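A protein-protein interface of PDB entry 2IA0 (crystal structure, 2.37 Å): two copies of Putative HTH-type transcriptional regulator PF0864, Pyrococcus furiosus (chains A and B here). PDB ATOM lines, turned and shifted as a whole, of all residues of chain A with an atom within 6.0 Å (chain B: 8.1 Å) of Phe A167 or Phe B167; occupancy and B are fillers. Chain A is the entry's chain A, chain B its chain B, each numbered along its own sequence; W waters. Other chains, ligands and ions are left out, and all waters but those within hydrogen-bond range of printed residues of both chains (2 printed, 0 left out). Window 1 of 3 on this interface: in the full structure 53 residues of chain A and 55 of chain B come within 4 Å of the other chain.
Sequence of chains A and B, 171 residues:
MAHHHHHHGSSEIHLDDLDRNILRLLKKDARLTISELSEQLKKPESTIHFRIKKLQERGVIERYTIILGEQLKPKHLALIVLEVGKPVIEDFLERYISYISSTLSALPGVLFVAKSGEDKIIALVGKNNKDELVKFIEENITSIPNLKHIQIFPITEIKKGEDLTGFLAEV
Of the 24 printed residues of chain B, 14 touch a printed residue of chain A.
Hydrophobic or aromatic side chains of chain B that line the printed part of chain A: Tyr B64, Ile B66, Ile B67, Phe B112, Leu B164 and Phe B167.
Hydrophobic or aromatic side chains of chain A within 4 Å of the printed part of chain B: Ile A66, Ile A67, Leu A164 and Phe A167.
Among the printed residues, 34 pairs touch across the chains.
N of Leu A68 lies within hydrogen-bond range of O of Gly A166 (2.9 Å).
OG1 of Thr B65 lies within hydrogen-bond range of O of Lys A27, at 2.8 Å.
The backbone carbonyl oxygen (O) of Phe B167 is in hydrogen-bond range of the side-chain amino group (NZ) of Lys A27 (3.2 Å).
The backbone carbonyl oxygen (O) of Ala B169 lies within hydrogen-bond range of the side-chain amino group (NZ) of Lys A27, at 2.8 Å.
O of Lys B27 is in hydrogen-bond range of NH1 of Arg A63, at 2.6 Å.
NH1 of Arg A63 lies within hydrogen-bond range of O of Lys B28 (3.1 Å).
O of Arg A63 sits at hydrogen-bond distance from N of Ile B67 (2.6 Å).
The side-chain carboxylate of Asp B163 is in salt-bridge range of the guanidinium group of Arg A63, at 2.5 Å.
The side-chain hydroxyl (OG1) of Thr A65 is in hydrogen-bond range of the backbone carbonyl oxygen (O) of Lys B27.
N of Thr A65 lies within hydrogen-bond range of O of Thr B65, 2.9 Å away.
O of Ile A67 is in hydrogen-bond range of N of Glu B62, at 2.9 Å.
N of Ile A67 is in hydrogen-bond range of O of Arg B63 (2.8 Å).
OD2 of Asp A163 is in salt-bridge range of NH1 of Arg B63, at 2.5 Å.
O of Phe A167 sits at hydrogen-bond distance from NZ of Lys B27 (3.3 Å).
The backbone carbonyl oxygen of Ala A169 sits at hydrogen-bond distance from the side-chain amino group of Lys B27 (2.5 Å).
The side-chain carboxylate of Asp A163 lies close to the side-chain carboxylate of Glu B62, 3.0 Å away.
Of the printed residues of chain B, Thr A65 touches Lys B27 (2.6 Å), Tyr B64 (3.5 Å), Thr B65 (2.9 Å) and Ile B67 (3.7 Å).
Of the printed residues of chain A, Ile B66 touches Lys A27 (3.8 Å) and Arg A63 (3.2 Å).
The nearest residue of chain A that does not touch Phe B167 is Thr A65 (5.4 Å).
The nearest printed residue of chain B that does not touch Leu A68 is Lys B27 (4.1 Å).
Lys A27 touches Thr B65, and with the chains exchanged Thr A65 touches Lys B27.
Asp A163 touches Phe B167, and with the chains exchanged Phe A167 touches Asp B163.
Leu A164 touches its own counterpart, Leu B164.
Positions printed for both chains: 27, 63, 65, 66, 67, 68, 161, 163, 164, 165, 166, 167, 168 and 169.
Water W2 lies within hydrogen-bond range of the side-chain amino group of Lys A27 (2.8 Å) and the backbone carbonyl oxygen of Phe B167 (3.4 Å).
Water W1 lies within hydrogen-bond range of O of Phe A167 (2.8 Å), OG1 of Thr A65 (2.9 Å), O of Ile A66 (3.3 Å) and NZ of Lys B27 (3.4 Å).
Thr A65 touches Ile B67.
Ile A67 touches Thr B65.
Phe B167 touches Asp A163 (CZ to O, 3.7 Å).
Leu A164 touches Phe B112 (CD1 to CD1, 3.8 Å).
Leu A164 touches Phe B167 (N to CE2, 3.7 Å).
CB of Asp B163 touches CZ of Phe A167 (3.6 Å).
Phe A167 touches Leu B164 (CE2 to N, 3.99 Å).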
ATOM      1  N   LYS A  27      -1.452  19.071 -21.078  1.00  0.00           N
ATOM      2  CA  LYS A  27      -1.507  17.955 -22.022  1.00  0.00           C
ATOM      3  C   LYS A  27      -2.038  16.738 -21.292  1.00  0.00           C
ATOM      4  O   LYS A  27      -2.965  16.108 -21.767  1.00  0.00           O
ATOM      5  CB  LYS A  27      -0.114  17.625 -22.594  1.00  0.00           C
ATOM      6  CG  LYS A  27       0.276  18.403 -23.840  1.00  0.00           C
ATOM      7  CD  LYS A  27       1.710  18.093 -24.316  1.00  0.00           C
ATOM      8  CE  LYS A  27       1.810  16.669 -24.874  1.00  0.00           C
ATOM      9  NZ  LYS A  27       0.932  16.502 -26.073  1.00  0.00           N
ATOM     10  N   ARG A  63      -4.916  25.248 -28.773  1.00  0.00           N
ATOM     11  CA  ARG A  63      -6.339  24.933 -28.675  1.00  0.00           C
ATOM     12  C   ARG A  63      -6.558  23.938 -27.560  1.00  0.00           C
ATOM     13  O   ARG A  63      -5.678  23.158 -27.284  1.00  0.00           O
ATOM     14  CB  ARG A  63      -6.821  24.330 -30.010  1.00  0.00           C
ATOM     15  CG  ARG A  63      -8.326  24.136 -30.151  1.00  0.00           C
ATOM     16  CD  ARG A  63      -8.754  24.306 -31.613  1.00  0.00           C
ATOM     17  NE  ARG A  63      -8.430  23.116 -32.386  1.00  0.00           N
ATOM     18  CZ  ARG A  63      -9.054  21.954 -32.217  1.00  0.00           C
ATOM     19  NH1 ARG A  63     -10.027  21.847 -31.314  1.00  0.00           N
ATOM     20  NH2 ARG A  63      -8.712  20.904 -32.940  1.00  0.00           N
ATOM     21  N   THR A  65      -9.065  20.816 -26.392  1.00  0.00           N
ATOM     22  CA  THR A  65      -9.995  19.879 -27.006  1.00  0.00           C
ATOM     23  C   THR A  65     -10.320  18.667 -26.087  1.00  0.00           C
ATOM     24  O   THR A  65      -9.793  18.540 -24.969  1.00  0.00           O
ATOM     25  CB  THR A  65      -9.497  19.480 -28.449  1.00  0.00           C
ATOM     26  OG1 THR A  65     -10.494  18.699 -29.130  1.00  0.00           O
ATOM     27  CG2 THR A  65      -8.201  18.718 -28.390  1.00  0.00           C
ATOM     28  N   ILE A  66     -11.229  17.816 -26.536  1.00  0.00           N
ATOM     29  CA  ILE A  66     -11.513  16.567 -25.841  1.00  0.00           C
ATOM     30  C   ILE A  66     -11.136  15.355 -26.700  1.00  0.00           C
ATOM     31  O   ILE A  66     -10.968  15.447 -27.919  1.00  0.00           O
ATOM     32  CB  ILE A  66     -12.992  16.453 -25.390  1.00  0.00           C
ATOM     33  CG1 ILE A  66     -13.911  16.559 -26.608  1.00  0.00           C
ATOM     34  CG2 ILE A  66     -13.314  17.481 -24.268  1.00  0.00           C
ATOM     35  CD1 ILE A  66     -15.219  15.834 -26.439  1.00  0.00           C
ATOM     36  N   ILE A  67     -10.953  14.233 -26.017  1.00  0.00           N
ATOM     37  CA  ILE A  67     -10.628  12.959 -26.626  1.00  0.00           C
ATOM     38  C   ILE A  67     -11.863  12.121 -26.406  1.00  0.00           C
ATOM     39  O   ILE A  67     -12.370  12.057 -25.289  1.00  0.00           O
ATOM     40  CB  ILE A  67      -9.379  12.337 -25.941  1.00  0.00           C
ATOM     41  CG1 ILE A  67      -8.120  13.028 -26.468  1.00  0.00           C
ATOM     42  CG2 ILE A  67      -9.277  10.809 -26.205  1.00  0.00           C
ATOM     43  CD1 ILE A  67      -7.015  13.022 -25.500  1.00  0.00           C
ATOM     44  N   LEU A  68     -12.369  11.513 -27.469  1.00  0.00           N
ATOM     45  CA  LEU A  68     -13.611  10.729 -27.388  1.00  0.00           C
ATOM     46  C   LEU A  68     -13.373   9.298 -26.882  1.00  0.00           C
ATOM     47  O   LEU A  68     -12.295   8.741 -27.063  1.00  0.00           O
ATOM     48  CB  LEU A  68     -14.316  10.716 -28.744  1.00  0.00           C
ATOM     49  CG  LEU A  68     -14.920  12.044 -29.200  1.00  0.00           C
ATOM     50  CD1 LEU A  68     -15.733  11.860 -30.435  1.00  0.00           C
ATOM     51  CD2 LEU A  68     -15.770  12.641 -28.100  1.00  0.00           C
ATOM     52  N   GLY A 161       0.842   6.735 -28.901  1.00  0.00           N
ATOM     53  CA  GLY A 161      -0.204   7.571 -29.494  1.00  0.00           C
ATOM     54  C   GLY A 161      -1.607   6.964 -29.589  1.00  0.00           C
ATOM     55  O   GLY A 161      -2.353   7.303 -30.503  1.00  0.00           O
ATOM     56  N   ASP A 163      -4.383   7.538 -28.044  1.00  0.00           N
ATOM     57  CA  ASP A 163      -5.456   8.519 -28.022  1.00  0.00           C
ATOM     58  C   ASP A 163      -5.652   9.346 -29.307  1.00  0.00           C
ATOM     59  O   ASP A 163      -6.591  10.126 -29.366  1.00  0.00           O
ATOM     60  CB  ASP A 163      -5.374   9.375 -26.758  1.00  0.00           C
ATOM     61  CG  ASP A 163      -5.499   8.542 -25.503  1.00  0.00           C
ATOM     62  OD1 ASP A 163      -6.371   7.621 -25.465  1.00  0.00           O
ATOM     63  OD2 ASP A 163      -4.713   8.782 -24.563  1.00  0.00           O
ATOM     64  N   LEU A 164      -4.798   9.147 -30.322  1.00  0.00           N
ATOM     65  CA  LEU A 164      -4.989   9.708 -31.701  1.00  0.00           C
ATOM     66  C   LEU A 164      -6.389   9.488 -32.262  1.00  0.00           C
ATOM     67  O   LEU A 164      -6.987  10.404 -32.822  1.00  0.00           O
ATOM     68  CB  LEU A 164      -3.943   9.134 -32.700  1.00  0.00           C
ATOM     69  CG  LEU A 164      -4.119   9.116 -34.251  1.00  0.00           C
ATOM     70  CD1 LEU A 164      -2.790   9.309 -34.988  1.00  0.00           C
ATOM     71  CD2 LEU A 164      -4.839   7.830 -34.832  1.00  0.00           C
ATOM     72  N   THR A 165      -6.912   8.273 -32.117  1.00  0.00           N
ATOM     73  CA  THR A 165      -8.206   7.942 -32.716  1.00  0.00           C
ATOM     74  C   THR A 165      -9.425   8.508 -31.948  1.00  0.00           C
ATOM     75  O   THR A 165     -10.450   8.825 -32.556  1.00  0.00           O
ATOM     76  CB  THR A 165      -8.324   6.425 -33.072  1.00  0.00           C
ATOM     77  OG1 THR A 165      -9.677   6.100 -33.451  1.00  0.00           O
ATOM     78  CG2 THR A 165      -7.861   5.565 -31.907  1.00  0.00           C
ATOM     79  N   GLY A 166      -9.289   8.675 -30.634  1.00  0.00           N
ATOM     80  CA  GLY A 166     -10.218   9.489 -29.860  1.00  0.00           C
ATOM     81  C   GLY A 166     -10.127  10.979 -30.175  1.00  0.00           C
ATOM     82  O   GLY A 166     -11.117  11.697 -30.131  1.00  0.00           O
ATOM     83  N   PHE A 167      -8.936  11.463 -30.469  1.00  0.00           N
ATOM     84  CA  PHE A 167      -8.788  12.840 -30.918  1.00  0.00           C
ATOM     85  C   PHE A 167      -9.419  13.130 -32.318  1.00  0.00           C
ATOM     86  O   PHE A 167     -10.124  14.126 -32.492  1.00  0.00           O
ATOM     87  CB  PHE A 167      -7.307  13.261 -30.858  1.00  0.00           C
ATOM     88  CG  PHE A 167      -7.052  14.623 -31.427  1.00  0.00           C
ATOM     89  CD1 PHE A 167      -7.542  15.766 -30.780  1.00  0.00           C
ATOM     90  CD2 PHE A 167      -6.357  14.767 -32.636  1.00  0.00           C
ATOM     91  CE1 PHE A 167      -7.334  17.045 -31.330  1.00  0.00           C
ATOM     92  CE2 PHE A 167      -6.140  16.020 -33.186  1.00  0.00           C
ATOM     93  CZ  PHE A 167      -6.633  17.170 -32.530  1.00  0.00           C
ATOM     94  N   LEU A 168      -9.156  12.260 -33.300  1.00  0.00           N
ATOM     95  CA  LEU A 168      -9.584  12.463 -34.684  1.00  0.00           C
ATOM     96  C   LEU A 168     -11.016  11.989 -34.952  1.00  0.00           C
ATOM     97  O   LEU A 168     -11.611  12.360 -35.982  1.00  0.00           O
ATOM     98  CB  LEU A 168      -8.616  11.743 -35.656  1.00  0.00           C
ATOM     99  CG  LEU A 168      -7.165  12.214 -35.726  1.00  0.00           C
ATOM    100  CD1 LEU A 168      -6.304  11.307 -36.613  1.00  0.00           C
ATOM    101  CD2 LEU A 168      -7.069  13.659 -36.182  1.00  0.00           C
ATOM    102  N   ALA A 169     -11.548  11.157 -34.059  1.00  0.00           N
ATOM    103  CA  ALA A 169     -12.905  10.610 -34.192  1.00  0.00           C
ATOM    104  C   ALA A 169     -13.886  11.728 -34.455  1.00  0.00           C
ATOM    105  O   ALA A 169     -13.912  12.734 -33.738  1.00  0.00           O
ATOM    106  CB  ALA A 169     -13.318   9.846 -32.921  1.00  0.00           C
ATOM    107  N   LYS B  27     -15.107  19.598 -28.747  1.00  0.00           N
ATOM    108  CA  LYS B  27     -13.975  19.240 -29.609  1.00  0.00           C
ATOM    109  C   LYS B  27     -13.245  20.435 -30.220  1.00  0.00           C
ATOM    110  O   LYS B  27     -12.034  20.379 -30.412  1.00  0.00           O
ATOM    111  CB  LYS B  27     -14.412  18.271 -30.711  1.00  0.00           C
ATOM    112  CG  LYS B  27     -14.291  16.817 -30.301  1.00  0.00           C
ATOM    113  CD  LYS B  27     -15.139  15.895 -31.164  1.00  0.00           C
ATOM    114  CE  LYS B  27     -14.568  15.702 -32.581  1.00  0.00           C
ATOM    115  NZ  LYS B  27     -13.309  14.890 -32.599  1.00  0.00           N
ATOM    116  N   LYS B  28     -13.995  21.486 -30.542  1.00  0.00           N
ATOM    117  CA  LYS B  28     -13.471  22.750 -31.053  1.00  0.00           C
ATOM    118  C   LYS B  28     -12.851  23.593 -29.930  1.00  0.00           C
ATOM    119  O   LYS B  28     -11.750  24.140 -30.097  1.00  0.00           O
ATOM    120  CB  LYS B  28     -14.616  23.536 -31.667  1.00  0.00           C
ATOM    121  CG  LYS B  28     -14.730  23.488 -33.180  1.00  0.00           C
ATOM    122  CD  LYS B  28     -16.195  23.333 -33.644  1.00  0.00           C
ATOM    123  CE  LYS B  28     -17.044  24.621 -33.535  1.00  0.00           C
ATOM    124  NZ  LYS B  28     -18.117  24.665 -34.646  1.00  0.00           N
ATOM    125  N   GLU B  62     -13.450  11.173 -22.698  1.00  0.00           N
ATOM    126  CA  GLU B  62     -12.483  10.372 -21.990  1.00  0.00           C
ATOM    127  C   GLU B  62     -11.527  11.289 -21.244  1.00  0.00           C
ATOM    128  O   GLU B  62     -11.123  11.003 -20.094  1.00  0.00           O
ATOM    129  CB  GLU B  62     -11.737   9.475 -22.977  1.00  0.00           C
ATOM    130  CG  GLU B  62     -10.546   8.750 -22.372  1.00  0.00           C
ATOM    131  CD  GLU B  62      -9.765   7.913 -23.375  1.00  0.00           C
ATOM    132  OE1 GLU B  62     -10.384   7.093 -24.101  1.00  0.00           O
ATOM    133  OE2 GLU B  62      -8.511   8.066 -23.413  1.00  0.00           O
ATOM    134  N   ARG B  63     -11.195  12.407 -21.889  1.00  0.00           N
ATOM    135  CA  ARG B  63     -10.077  13.239 -21.473  1.00  0.00           C
ATOM    136  C   ARG B  63     -10.136  14.603 -22.129  1.00  0.00           C
ATOM    137  O   ARG B  63     -10.537  14.708 -23.282  1.00  0.00           O
ATOM    138  CB  ARG B  63      -8.743  12.550 -21.841  1.00  0.00           C
ATOM    139  CG  ARG B  63      -7.612  12.892 -20.874  1.00  0.00           C
ATOM    140  CD  ARG B  63      -6.357  12.090 -21.141  1.00  0.00           C
ATOM    141  NE  ARG B  63      -5.453  12.779 -22.070  1.00  0.00           N
ATOM    142  CZ  ARG B  63      -4.867  12.188 -23.103  1.00  0.00           C
ATOM    143  NH1 ARG B  63      -5.098  10.917 -23.343  1.00  0.00           N
ATOM    144  NH2 ARG B  63      -4.061  12.860 -23.908  1.00  0.00           N
ATOM    145  N   TYR B  64      -9.748  15.633 -21.364  1.00  0.00           N
ATOM    146  CA  TYR B  64      -9.501  17.011 -21.843  1.00  0.00           C
ATOM    147  C   TYR B  64      -7.997  17.227 -22.005  1.00  0.00           C
ATOM    148  O   TYR B  64      -7.207  16.930 -21.109  1.00  0.00           O
ATOM    149  CB  TYR B  64     -10.026  18.040 -20.839  1.00  0.00           C
ATOM    150  CG  TYR B  64     -11.513  18.046 -20.694  1.00  0.00           C
ATOM    151  CD1 TYR B  64     -12.259  19.123 -21.123  1.00  0.00           C
ATOM    152  CD2 TYR B  64     -12.180  16.962 -20.133  1.00  0.00           C
ATOM    153  CE1 TYR B  64     -13.632  19.121 -21.022  1.00  0.00           C
ATOM    154  CE2 TYR B  64     -13.564  16.963 -19.997  1.00  0.00           C
ATOM    155  CZ  TYR B  64     -14.283  18.041 -20.457  1.00  0.00           C
ATOM    156  OH  TYR B  64     -15.651  18.039 -20.349  1.00  0.00           O
ATOM    157  N   THR B  65      -7.599  17.755 -23.150  1.00  0.00           N
ATOM    158  CA  THR B  65      -6.188  17.995 -23.424  1.00  0.00           C
ATOM    159  C   THR B  65      -6.018  19.309 -24.211  1.00  0.00           C
ATOM    160  O   THR B  65      -7.002  20.011 -24.468  1.00  0.00           O
ATOM    161  CB  THR B  65      -5.587  16.764 -24.161  1.00  0.00           C
ATOM    162  OG1 THR B  65      -4.158  16.846 -24.176  1.00  0.00           O
ATOM    163  CG2 THR B  65      -6.140  16.632 -25.582  1.00  0.00           C
ATOM    164  N   ILE B  66      -4.780  19.617 -24.611  1.00  0.00           N
ATOM    165  CA  ILE B  66      -4.485  20.800 -25.419  1.00  0.00           C
ATOM    166  C   ILE B  66      -3.778  20.420 -26.715  1.00  0.00           C
ATOM    167  O   ILE B  66      -3.102  19.388 -26.797  1.00  0.00           O
ATOM    168  CB  ILE B  66      -3.581  21.857 -24.650  1.00  0.00           C
ATOM    169  CG1 ILE B  66      -2.269  21.230 -24.156  1.00  0.00           C
ATOM    170  CG2 ILE B  66      -4.361  22.577 -23.521  1.00  0.00           C
ATOM    171  CD1 ILE B  66      -1.188  22.242 -23.817  1.00  0.00           C
ATOM    172  N   ILE B  67      -3.935  21.256 -27.730  1.00  0.00           N
ATOM    173  CA  ILE B  67      -3.137  21.154 -28.942  1.00  0.00           C
ATOM    174  C   ILE B  67      -2.023  22.190 -28.852  1.00  0.00           C
ATOM    175  O   ILE B  67      -2.285  23.356 -28.516  1.00  0.00           O
ATOM    176  CB  ILE B  67      -4.032  21.299 -30.232  1.00  0.00           C
ATOM    177  CG1 ILE B  67      -4.969  20.083 -30.342  1.00  0.00           C
ATOM    178  CG2 ILE B  67      -3.175  21.339 -31.510  1.00  0.00           C
ATOM    179  CD1 ILE B  67      -6.204  20.393 -31.048  1.00  0.00           C
ATOM    180  N   LEU B  68      -0.782  21.730 -29.046  1.00  0.00           N
ATOM    181  CA  LEU B  68       0.410  22.590 -29.141  1.00  0.00           C
ATOM    182  C   LEU B  68       0.579  23.201 -30.547  1.00  0.00           C
ATOM    183  O   LEU B  68       0.209  22.595 -31.557  1.00  0.00           O
ATOM    184  CB  LEU B  68       1.676  21.812 -28.774  1.00  0.00           C
ATOM    185  CG  LEU B  68       1.772  21.068 -27.434  1.00  0.00           C
ATOM    186  CD1 LEU B  68       3.102  20.323 -27.415  1.00  0.00           C
ATOM    187  CD2 LEU B  68       1.606  21.993 -26.183  1.00  0.00           C
ATOM    188  N   GLY B  69       1.137  24.402 -30.628  1.00  0.00           N
ATOM    189  CA  GLY B  69       1.277  25.033 -31.933  1.00  0.00           C
ATOM    190  C   GLY B  69       2.709  25.388 -32.245  1.00  0.00           C
ATOM    191  O   GLY B  69       3.638  24.784 -31.717  1.00  0.00           O
ATOM    192  N   LEU B  72       6.599  24.231 -31.151  1.00  0.00           N
ATOM    193  CA  LEU B  72       6.617  22.881 -30.567  1.00  0.00           C
ATOM    194  C   LEU B  72       6.074  21.748 -31.454  1.00  0.00           C
ATOM    195  O   LEU B  72       6.139  20.578 -31.057  1.00  0.00           O
ATOM    196  CB  LEU B  72       5.959  22.851 -29.178  1.00  0.00           C
ATOM    197  CG  LEU B  72       6.665  23.585 -28.034  1.00  0.00           C
ATOM    198  CD1 LEU B  72       5.683  23.909 -26.915  1.00  0.00           C
ATOM    199  CD2 LEU B  72       7.839  22.770 -27.500  1.00  0.00           C
ATOM    200  N   LYS B  73       5.537  22.083 -32.631  1.00  0.00           N
ATOM    201  CA  LYS B  73       5.256  21.075 -33.664  1.00  0.00           C
ATOM    202  C   LYS B  73       6.551  20.880 -34.452  1.00  0.00           C
ATOM    203  O   LYS B  73       7.130  21.869 -34.922  1.00  0.00           O
ATOM    204  CB  LYS B  73       4.189  21.531 -34.672  1.00  0.00           C
ATOM    205  CG  LYS B  73       2.756  21.746 -34.197  1.00  0.00           C
ATOM    206  CD  LYS B  73       1.887  22.069 -35.438  1.00  0.00           C
ATOM    207  CE  LYS B  73       0.806  23.147 -35.187  1.00  0.00           C
ATOM    208  NZ  LYS B  73      -0.334  22.755 -34.271  1.00  0.00           N
ATOM    209  N   LEU B 111       6.429  10.076 -32.602  1.00  0.00           N
ATOM    210  CA  LEU B 111       5.144  10.607 -32.142  1.00  0.00           C
ATOM    211  C   LEU B 111       4.069   9.548 -32.073  1.00  0.00           C
ATOM    212  O   LEU B 111       3.141   9.656 -31.285  1.00  0.00           O
ATOM    213  CB  LEU B 111       4.660  11.726 -33.074  1.00  0.00           C
ATOM    214  CG  LEU B 111       5.607  12.827 -33.559  1.00  0.00           C
ATOM    215  CD1 LEU B 111       4.792  13.795 -34.336  1.00  0.00           C
ATOM    216  CD2 LEU B 111       6.272  13.536 -32.394  1.00  0.00           C
ATOM    217  N   PHE B 112       4.212   8.533 -32.911  1.00  0.00           N
ATOM    218  CA  PHE B 112       3.197   7.528 -33.114  1.00  0.00           C
ATOM    219  C   PHE B 112       3.896   6.221 -33.484  1.00  0.00           C
ATOM    220  O   PHE B 112       4.767   6.221 -34.340  1.00  0.00           O
ATOM    221  CB  PHE B 112       2.270   7.949 -34.252  1.00  0.00           C
ATOM    222  CG  PHE B 112       1.203   6.940 -34.561  1.00  0.00           C
ATOM    223  CD1 PHE B 112      -0.002   6.933 -33.839  1.00  0.00           C
ATOM    224  CD2 PHE B 112       1.409   5.975 -35.538  1.00  0.00           C
ATOM    225  CE1 PHE B 112      -0.978   5.982 -34.098  1.00  0.00           C
ATOM    226  CE2 PHE B 112       0.439   5.019 -35.799  1.00  0.00           C
ATOM    227  CZ  PHE B 112      -0.749   5.019 -35.089  1.00  0.00           C
ATOM    228  N   GLY B 161      -6.727  16.846 -40.776  1.00  0.00           N
ATOM    229  CA  GLY B 161      -6.074  16.408 -39.533  1.00  0.00           C
ATOM    230  C   GLY B 161      -4.776  17.113 -39.191  1.00  0.00           C
ATOM    231  O   GLY B 161      -3.923  16.543 -38.515  1.00  0.00           O
ATOM    232  N   GLU B 162      -4.617  18.349 -39.648  1.00  0.00           N
ATOM    233  CA  GLU B 162      -3.403  19.145 -39.402  1.00  0.00           C
ATOM    234  C   GLU B 162      -3.017  19.194 -37.927  1.00  0.00           C
ATOM    235  O   GLU B 162      -1.836  19.212 -37.606  1.00  0.00           O
ATOM    236  CB  GLU B 162      -3.622  20.591 -39.864  1.00  0.00           C
ATOM    237  CG  GLU B 162      -3.476  20.851 -41.331  1.00  0.00           C
ATOM    238  CD  GLU B 162      -4.192  22.130 -41.745  1.00  0.00           C
ATOM    239  OE1 GLU B 162      -4.436  22.994 -40.853  1.00  0.00           O
ATOM    240  OE2 GLU B 162      -4.521  22.264 -42.958  1.00  0.00           O
ATOM    241  N   ASP B 163      -4.028  19.247 -37.048  1.00  0.00           N
ATOM    242  CA  ASP B 163      -3.853  19.323 -35.584  1.00  0.00           C
ATOM    243  C   ASP B 163      -3.228  18.106 -34.926  1.00  0.00           C
ATOM    244  O   ASP B 163      -2.854  18.171 -33.755  1.00  0.00           O
ATOM    245  CB  ASP B 163      -5.199  19.550 -34.895  1.00  0.00           C
ATOM    246  CG  ASP B 163      -5.723  20.930 -35.090  1.00  0.00           C
ATOM    247  OD1 ASP B 163      -5.028  21.760 -35.719  1.00  0.00           O
ATOM    248  OD2 ASP B 163      -6.844  21.182 -34.613  1.00  0.00           O
ATOM    249  N   LEU B 164      -3.169  17.000 -35.661  1.00  0.00           N
ATOM    250  CA  LEU B 164      -2.593  15.752 -35.185  1.00  0.00           C
ATOM    251  C   LEU B 164      -1.178  15.929 -34.655  1.00  0.00           C
ATOM    252  O   LEU B 164      -0.854  15.395 -33.610  1.00  0.00           O
ATOM    253  CB  LEU B 164      -2.637  14.695 -36.299  1.00  0.00           C
ATOM    254  CG  LEU B 164      -1.764  13.439 -36.233  1.00  0.00           C
ATOM    255  CD1 LEU B 164      -2.357  12.339 -37.098  1.00  0.00           C
ATOM    256  CD2 LEU B 164      -0.303  13.709 -36.660  1.00  0.00           C
ATOM    257  N   THR B 165      -0.342  16.664 -35.381  1.00  0.00           N
ATOM    258  CA  THR B 165       1.036  16.928 -34.944  1.00  0.00           C
ATOM    259  C   THR B 165       1.093  17.633 -33.577  1.00  0.00           C
ATOM    260  O   THR B 165       1.768  17.163 -32.677  1.00  0.00           O
ATOM    261  CB  THR B 165       1.814  17.792 -35.971  1.00  0.00           C
ATOM    262  OG1 THR B 165       1.681  17.224 -37.276  1.00  0.00           O
ATOM    263  CG2 THR B 165       3.272  17.843 -35.611  1.00  0.00           C
ATOM    264  N   GLY B 166       0.379  18.755 -33.452  1.00  0.00           N
ATOM    265  CA  GLY B 166       0.258  19.514 -32.209  1.00  0.00           C
ATOM    266  C   GLY B 166      -0.304  18.674 -31.086  1.00  0.00           C
ATOM    267  O   GLY B 166       0.040  18.865 -29.939  1.00  0.00           O
ATOM    268  N   PHE B 167      -1.158  17.717 -31.431  1.00  0.00           N
ATOM    269  CA  PHE B 167      -1.710  16.807 -30.444  1.00  0.00           C
ATOM    270  C   PHE B 167      -0.687  15.783 -29.964  1.00  0.00           C
ATOM    271  O   PHE B 167      -0.569  15.544 -28.770  1.00  0.00           O
ATOM    272  CB  PHE B 167      -2.947  16.092 -30.990  1.00  0.00           C
ATOM    273  CG  PHE B 167      -3.425  14.969 -30.105  1.00  0.00           C
ATOM    274  CD1 PHE B 167      -4.070  15.239 -28.906  1.00  0.00           C
ATOM    275  CD2 PHE B 167      -3.190  13.634 -30.458  1.00  0.00           C
ATOM    276  CE1 PHE B 167      -4.484  14.190 -28.066  1.00  0.00           C
ATOM    277  CE2 PHE B 167      -3.596  12.584 -29.632  1.00  0.00           C
ATOM    278  CZ  PHE B 167      -4.251  12.858 -28.441  1.00  0.00           C
ATOM    279  N   LEU B 168       0.032  15.165 -30.902  1.00  0.00           N
ATOM    280  CA  LEU B 168       0.978  14.106 -30.559  1.00  0.00           C
ATOM    281  C   LEU B 168       2.303  14.641 -30.064  1.00  0.00           C
ATOM    282  O   LEU B 168       3.062  13.911 -29.422  1.00  0.00           O
ATOM    283  CB  LEU B 168       1.221  13.193 -31.749  1.00  0.00           C
ATOM    284  CG  LEU B 168       0.057  12.353 -32.264  1.00  0.00           C
ATOM    285  CD1 LEU B 168       0.550  11.658 -33.521  1.00  0.00           C
ATOM    286  CD2 LEU B 168      -0.458  11.342 -31.237  1.00  0.00           C
ATOM    287  N   ALA B 169       2.583  15.906 -30.360  1.00  0.00           N
ATOM    288  CA  ALA B 169       3.879  16.478 -30.046  1.00  0.00           C
ATOM    289  C   ALA B 169       4.111  16.528 -28.532  1.00  0.00           C
ATOM    290  O   ALA B 169       3.198  16.854 -27.763  1.00  0.00           O
ATOM    291  CB  ALA B 169       4.007  17.861 -30.668  1.00  0.00           C
ATOM    292  N   GLU B 170       5.327  16.197 -28.104  1.00  0.00           N
ATOM    293  CA  GLU B 170       5.616  16.177 -26.667  1.00  0.00           C
ATOM    294  C   GLU B 170       6.454  17.375 -26.126  1.00  0.00           C
ATOM    295  O   GLU B 170       7.077  18.120 -26.881  1.00  0.00           O
ATOM    296  CB  GLU B 170       6.186  14.800 -26.246  1.00  0.00           C
ATOM    297  CG  GLU B 170       6.195  14.541 -24.705  1.00  0.00           C
ATOM    298  CD  GLU B 170       4.809  14.656 -24.043  1.00  0.00           C
ATOM    299  OE1 GLU B 170       3.847  14.043 -24.575  1.00  0.00           O
ATOM    300  OE2 GLU B 170       4.690  15.346 -22.990  1.00  0.00           O
HETATM  301  O   HOH W   1     -10.702  16.465 -31.021  1.00  0.00           O
HETATM  302  O   HOH W   2       0.742  13.724 -26.250  1.00  0.00           O
